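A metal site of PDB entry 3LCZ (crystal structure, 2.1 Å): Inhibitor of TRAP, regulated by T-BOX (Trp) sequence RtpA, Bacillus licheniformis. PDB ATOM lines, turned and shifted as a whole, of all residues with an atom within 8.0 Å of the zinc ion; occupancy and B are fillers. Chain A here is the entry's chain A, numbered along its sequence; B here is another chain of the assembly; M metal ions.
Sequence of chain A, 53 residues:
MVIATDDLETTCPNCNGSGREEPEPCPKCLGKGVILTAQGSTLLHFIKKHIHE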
ATOM      1  N   THR A  10      30.904  24.227 -11.885  1.00  0.00           N
ATOM      2  CA  THR A  10      31.691  24.881 -12.924  1.00  0.00           C
ATOM      3  C   THR A  10      30.737  25.579 -13.900  1.00  0.00           C
ATOM      4  O   THR A  10      29.590  25.184 -14.052  1.00  0.00           O
ATOM      5  CB  THR A  10      32.689  23.919 -13.639  1.00  0.00           C
ATOM      6  OG1 THR A  10      32.382  23.726 -14.998  1.00  0.00           O
ATOM      7  CG2 THR A  10      32.835  22.635 -12.916  1.00  0.00           C
ATOM      8  N   THR A  11      31.193  26.682 -14.478  1.00  0.00           N
ATOM      9  CA  THR A  11      30.393  27.466 -15.379  1.00  0.00           C
ATOM     10  C   THR A  11      29.674  26.540 -16.347  1.00  0.00           C
ATOM     11  O   THR A  11      30.273  25.638 -16.912  1.00  0.00           O
ATOM     12  CB  THR A  11      31.260  28.436 -16.175  1.00  0.00           C
ATOM     13  OG1 THR A  11      32.051  29.217 -15.275  1.00  0.00           O
ATOM     14  CG2 THR A  11      30.381  29.375 -17.001  1.00  0.00           C
ATOM     15  N   CYS A  12      28.382  26.759 -16.510  1.00  0.00           N
ATOM     16  CA  CYS A  12      27.618  25.954 -17.422  1.00  0.00           C
ATOM     17  C   CYS A  12      28.073  26.248 -18.841  1.00  0.00           C
ATOM     18  O   CYS A  12      28.160  27.407 -19.250  1.00  0.00           O
ATOM     19  CB  CYS A  12      26.132  26.252 -17.249  1.00  0.00           C
ATOM     20  SG  CYS A  12      25.001  25.531 -18.420  1.00  0.00           S
ATOM     21  N   PRO A  13      28.275  25.176 -19.623  1.00  0.00           N
ATOM     22  CA  PRO A  13      28.783  25.401 -20.941  1.00  0.00           C
ATOM     23  C   PRO A  13      27.671  25.873 -21.883  1.00  0.00           C
ATOM     24  O   PRO A  13      27.975  26.452 -22.928  1.00  0.00           O
ATOM     25  CB  PRO A  13      29.258  24.009 -21.349  1.00  0.00           C
ATOM     26  CG  PRO A  13      28.260  23.106 -20.709  1.00  0.00           C
ATOM     27  CD  PRO A  13      27.978  23.753 -19.384  1.00  0.00           C
ATOM     28  N   ASN A  14      26.410  25.625 -21.531  1.00  0.00           N
ATOM     29  CA  ASN A  14      25.289  26.013 -22.411  1.00  0.00           C
ATOM     30  C   ASN A  14      24.946  27.492 -22.384  1.00  0.00           C
ATOM     31  O   ASN A  14      24.560  28.052 -23.384  1.00  0.00           O
ATOM     32  CB  ASN A  14      24.022  25.193 -22.168  1.00  0.00           C
ATOM     33  CG  ASN A  14      24.095  23.809 -22.780  1.00  0.00           C
ATOM     34  OD1 ASN A  14      24.935  22.999 -22.388  1.00  0.00           O
ATOM     35  ND2 ASN A  14      23.246  23.544 -23.776  1.00  0.00           N
ATOM     36  N   CYS A  15      25.094  28.122 -21.233  1.00  0.00           N
ATOM     37  CA  CYS A  15      24.723  29.518 -21.159  1.00  0.00           C
ATOM     38  C   CYS A  15      25.945  30.324 -20.841  1.00  0.00           C
ATOM     39  O   CYS A  15      25.877  31.536 -20.713  1.00  0.00           O
ATOM     40  CB  CYS A  15      23.668  29.730 -20.082  1.00  0.00           C
ATOM     41  SG  CYS A  15      24.241  29.152 -18.472  1.00  0.00           S
ATOM     42  N   ASN A  16      27.081  29.638 -20.741  1.00  0.00           N
ATOM     43  CA  ASN A  16      28.343  30.268 -20.322  1.00  0.00           C
ATOM     44  C   ASN A  16      28.233  31.078 -19.044  1.00  0.00           C
ATOM     45  O   ASN A  16      28.932  32.078 -18.889  1.00  0.00           O
ATOM     46  CB  ASN A  16      28.941  31.171 -21.404  1.00  0.00           C
ATOM     47  CG  ASN A  16      30.340  31.612 -21.032  1.00  0.00           C
ATOM     48  OD1 ASN A  16      31.134  30.824 -20.519  1.00  0.00           O
ATOM     49  ND2 ASN A  16      30.651  32.882 -21.284  1.00  0.00           N
ATOM     50  N   GLY A  17      27.334  30.693 -18.152  1.00  0.00           N
ATOM     51  CA  GLY A  17      27.269  31.375 -16.836  1.00  0.00           C
ATOM     52  C   GLY A  17      26.127  32.331 -16.592  1.00  0.00           C
ATOM     53  O   GLY A  17      25.868  32.699 -15.449  1.00  0.00           O
ATOM     54  N   SER A  18      25.381  32.704 -17.620  1.00  0.00           N
ATOM     55  CA  SER A  18      24.273  33.645 -17.428  1.00  0.00           C
ATOM     56  C   SER A  18      23.109  33.012 -16.659  1.00  0.00           C
ATOM     57  O   SER A  18      22.315  33.716 -15.979  1.00  0.00           O
ATOM     58  CB  SER A  18      23.770  34.155 -18.785  1.00  0.00           C
ATOM     59  OG  SER A  18      23.008  33.148 -19.450  1.00  0.00           O
ATOM     60  N   GLY A  19      22.999  31.690 -16.733  1.00  0.00           N
ATOM     61  CA  GLY A  19      21.840  31.000 -16.169  1.00  0.00           C
ATOM     62  C   GLY A  19      20.581  31.166 -17.051  1.00  0.00           C
ATOM     63  O   GLY A  19      19.501  30.752 -16.661  1.00  0.00           O
ATOM     64  N   ARG A  20      20.736  31.713 -18.255  1.00  0.00           N
ATOM     65  CA  ARG A  20      19.586  32.022 -19.130  1.00  0.00           C
ATOM     66  C   ARG A  20      19.669  31.445 -20.538  1.00  0.00           C
ATOM     67  O   ARG A  20      20.746  31.320 -21.110  1.00  0.00           O
ATOM     68  CB  ARG A  20      19.390  33.539 -19.280  1.00  0.00           C
ATOM     69  CG  ARG A  20      19.381  34.367 -17.984  1.00  0.00           C
ATOM     70  CD  ARG A  20      18.230  33.980 -17.062  1.00  0.00           C
ATOM     71  NE  ARG A  20      16.952  34.269 -17.693  1.00  0.00           N
ATOM     72  CZ  ARG A  20      15.777  33.817 -17.267  1.00  0.00           C
ATOM     73  NH1 ARG A  20      15.716  33.082 -16.175  1.00  0.00           N
ATOM     74  NH2 ARG A  20      14.673  34.141 -17.920  1.00  0.00           N
ATOM     75  N   GLU A  21      18.505  31.049 -21.040  1.00  0.00           N
ATOM     76  CA  GLU A  21      18.308  30.635 -22.422  1.00  0.00           C
ATOM     77  C   GLU A  21      16.981  31.301 -22.756  1.00  0.00           C
ATOM     78  O   GLU A  21      15.947  30.635 -22.845  1.00  0.00           O
ATOM     79  CB  GLU A  21      18.162  29.133 -22.531  1.00  0.00           C
ATOM     80  CG  GLU A  21      17.824  28.683 -23.923  1.00  0.00           C
ATOM     81  CD  GLU A  21      17.977  27.192 -24.079  1.00  0.00           C
ATOM     82  OE1 GLU A  21      19.024  26.687 -23.667  1.00  0.00           O
ATOM     83  OE2 GLU A  21      17.076  26.538 -24.661  1.00  0.00           O
ATOM     84  N   PRO A  25      14.894  30.117 -17.807  1.00  0.00           N
ATOM     85  CA  PRO A  25      16.157  29.810 -17.169  1.00  0.00           C
ATOM     86  C   PRO A  25      16.861  28.791 -18.054  1.00  0.00           C
ATOM     87  O   PRO A  25      16.200  28.085 -18.813  1.00  0.00           O
ATOM     88  CB  PRO A  25      15.726  29.187 -15.837  1.00  0.00           C
ATOM     89  CG  PRO A  25      14.299  28.810 -16.021  1.00  0.00           C
ATOM     90  CD  PRO A  25      13.749  29.822 -16.949  1.00  0.00           C
ATOM     91  N   CYS A  26      18.183  28.728 -18.043  1.00  0.00           N
ATOM     92  CA  CYS A  26      18.866  27.758 -18.904  1.00  0.00           C
ATOM     93  C   CYS A  26      18.530  26.381 -18.364  1.00  0.00           C
ATOM     94  O   CYS A  26      18.747  26.122 -17.163  1.00  0.00           O
ATOM     95  CB  CYS A  26      20.365  28.028 -18.820  1.00  0.00           C
ATOM     96  SG  CYS A  26      21.451  26.788 -19.573  1.00  0.00           S
ATOM     97  N   PRO A  27      18.068  25.461 -19.224  1.00  0.00           N
ATOM     98  CA  PRO A  27      17.646  24.163 -18.692  1.00  0.00           C
ATOM     99  C   PRO A  27      18.792  23.274 -18.248  1.00  0.00           C
ATOM    100  O   PRO A  27      18.592  22.378 -17.433  1.00  0.00           O
ATOM    101  CB  PRO A  27      16.893  23.530 -19.878  1.00  0.00           C
ATOM    102  CG  PRO A  27      17.447  24.187 -21.091  1.00  0.00           C
ATOM    103  CD  PRO A  27      17.946  25.527 -20.693  1.00  0.00           C
ATOM    104  N   LYS A  28      19.984  23.512 -18.787  1.00  0.00           N
ATOM    105  CA  LYS A  28      21.135  22.680 -18.469  1.00  0.00           C
ATOM    106  C   LYS A  28      21.639  22.955 -17.053  1.00  0.00           C
ATOM    107  O   LYS A  28      22.093  22.058 -16.367  1.00  0.00           O
ATOM    108  CB  LYS A  28      22.226  22.872 -19.517  1.00  0.00           C
ATOM    109  CG  LYS A  28      21.771  22.537 -20.958  1.00  0.00           C
ATOM    110  CD  LYS A  28      21.150  21.159 -21.057  1.00  0.00           C
ATOM    111  CE  LYS A  28      20.661  20.834 -22.476  1.00  0.00           C
ATOM    112  NZ  LYS A  28      19.332  21.441 -22.820  1.00  0.00           N
ATOM    113  N   CYS A  29      21.565  24.201 -16.594  1.00  0.00           N
ATOM    114  CA  CYS A  29      22.010  24.483 -15.228  1.00  0.00           C
ATOM    115  C   CYS A  29      20.849  24.897 -14.314  1.00  0.00           C
ATOM    116  O   CYS A  29      21.066  25.365 -13.189  1.00  0.00           O
ATOM    117  CB  CYS A  29      23.067  25.557 -15.239  1.00  0.00           C
ATOM    118  SG  CYS A  29      22.430  27.031 -15.978  1.00  0.00           S
ATOM    119  N   LEU A  30      19.624  24.734 -14.789  1.00  0.00           N
ATOM    120  CA  LEU A  30      18.458  25.113 -14.001  1.00  0.00           C
ATOM    121  C   LEU A  30      18.520  26.579 -13.612  1.00  0.00           C
ATOM    122  O   LEU A  30      18.070  26.937 -12.516  1.00  0.00           O
ATOM    123  CB  LEU A  30      18.354  24.248 -12.762  1.00  0.00           C
ATOM    124  CG  LEU A  30      18.193  22.758 -13.085  1.00  0.00           C
ATOM    125  CD1 LEU A  30      17.843  21.957 -11.837  1.00  0.00           C
ATOM    126  CD2 LEU A  30      17.108  22.570 -14.217  1.00  0.00           C
ATOM    127  N   GLY A  31      19.035  27.408 -14.509  1.00  0.00           N
ATOM    128  CA  GLY A  31      19.097  28.878 -14.288  1.00  0.00           C
ATOM    129  C   GLY A  31      20.211  29.337 -13.354  1.00  0.00           C
ATOM    130  O   GLY A  31      20.373  30.539 -13.073  1.00  0.00           O
ATOM    131  N   LYS A  32      20.981  28.378 -12.853  1.00  0.00           N
ATOM    132  CA  LYS A  32      22.065  28.676 -11.923  1.00  0.00           C
ATOM    133  C   LYS A  32      23.344  29.214 -12.592  1.00  0.00           C
ATOM    134  O   LYS A  32      24.140  29.870 -11.968  1.00  0.00           O
ATOM    135  CB  LYS A  32      22.404  27.415 -11.143  1.00  0.00           C
ATOM    136  CG  LYS A  32      21.749  27.295  -9.790  1.00  0.00           C
ATOM    137  CD  LYS A  32      20.260  27.493  -9.792  1.00  0.00           C
ATOM    138  CE  LYS A  32      19.697  27.103  -8.433  1.00  0.00           C
ATOM    139  NZ  LYS A  32      18.213  27.010  -8.445  1.00  0.00           N
ATOM    140  N   GLY A  33      23.558  28.869 -13.864  1.00  0.00           N
ATOM    141  CA  GLY A  33      24.777  29.331 -14.548  1.00  0.00           C
ATOM    142  C   GLY A  33      25.965  28.439 -14.290  1.00  0.00           C
ATOM    143  O   GLY A  33      27.039  28.636 -14.874  1.00  0.00           O
ATOM    144  N   VAL A  34      25.767  27.443 -13.419  1.00  0.00           N
ATOM    145  CA  VAL A  34      26.787  26.452 -13.082  1.00  0.00           C
ATOM    146  C   VAL A  34      26.207  25.036 -13.052  1.00  0.00           C
ATOM    147  O   VAL A  34      25.039  24.836 -12.747  1.00  0.00           O
ATOM    148  CB  VAL A  34      27.446  26.747 -11.715  1.00  0.00           C
ATOM    149  CG1 VAL A  34      28.285  28.030 -11.798  1.00  0.00           C
ATOM    150  CG2 VAL A  34      26.348  26.920 -10.618  1.00  0.00           C
ATOM    151  N   ILE A  35      27.052  24.056 -13.395  1.00  0.00           N
ATOM    152  CA  ILE A  35      26.694  22.660 -13.279  1.00  0.00           C
ATOM    153  C   ILE A  35      27.534  22.043 -12.173  1.00  0.00           C
ATOM    154  O   ILE A  35      28.614  22.531 -11.876  1.00  0.00           O
ATOM    155  CB  ILE A  35      26.793  21.925 -14.614  1.00  0.00           C
ATOM    156  CG1 ILE A  35      28.225  21.730 -15.078  1.00  0.00           C
ATOM    157  CG2 ILE A  35      25.905  22.615 -15.685  1.00  0.00           C
ATOM    158  CD1 ILE A  35      28.226  21.082 -16.477  1.00  0.00           C
ATOM    159  N   PRO B  13      26.458  18.488 -19.823  1.00  0.00           N
ATOM    160  CA  PRO B  13      25.039  18.609 -19.562  1.00  0.00           C
ATOM    161  C   PRO B  13      24.249  18.656 -20.854  1.00  0.00           C
ATOM    162  O   PRO B  13      23.063  18.280 -20.862  1.00  0.00           O
ATOM    163  CB  PRO B  13      24.939  19.965 -18.842  1.00  0.00           C
ATOM    164  CG  PRO B  13      26.079  20.737 -19.331  1.00  0.00           C
ATOM    165  CD  PRO B  13      27.174  19.756 -19.651  1.00  0.00           C
HETATM  166 ZN    ZN M   1      23.280  27.058 -18.138  1.00  0.00          ZN
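The zinc ion is bound by the side-chain sulfur of Cys 12 (2.3 Å), the side-chain sulfur of Cys 29 (2.3 Å), the side-chain sulfur of Cys 15 (2.3 Å) and the side-chain sulfur of Cys 26 (2.3 Å).
The zinc ion has four donor atoms within binding distance.
N of Asn 14 lies close to SG of Cys 12 (3.4 Å).
O of Gly 33 sits at hydrogen-bond distance from N of Cys 12.
The side-chain sulfur (SG) of Cys 29 sits close to the backbone NH (N) of Gly 33 (3.0 Å).
The side-chain sulfur (SG) of Cys 29 sits close to the backbone NH (N) of Gly 31 (3.7 Å).
The side-chain sulfur of Cys 29 sits close to the backbone NH of Lys 32, at 3.7 Å.
SG of Cys 15 lies close to N of Gly 19, 3.3 Å away.
The side-chain sulfur of Cys 26 sits close to the backbone NH of Lys 28 (3.7 Å).
The backbone carbonyl oxygen (O) of Cys 26 lies within hydrogen-bond range of the backbone NH (N) of Gly 31, 3.0 Å away.
Of the 24 residues printed, 4 come within 4 Å of the zinc ion.
Along chain A the residues within 4 Å of the zinc ion span positions 12 to 29.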
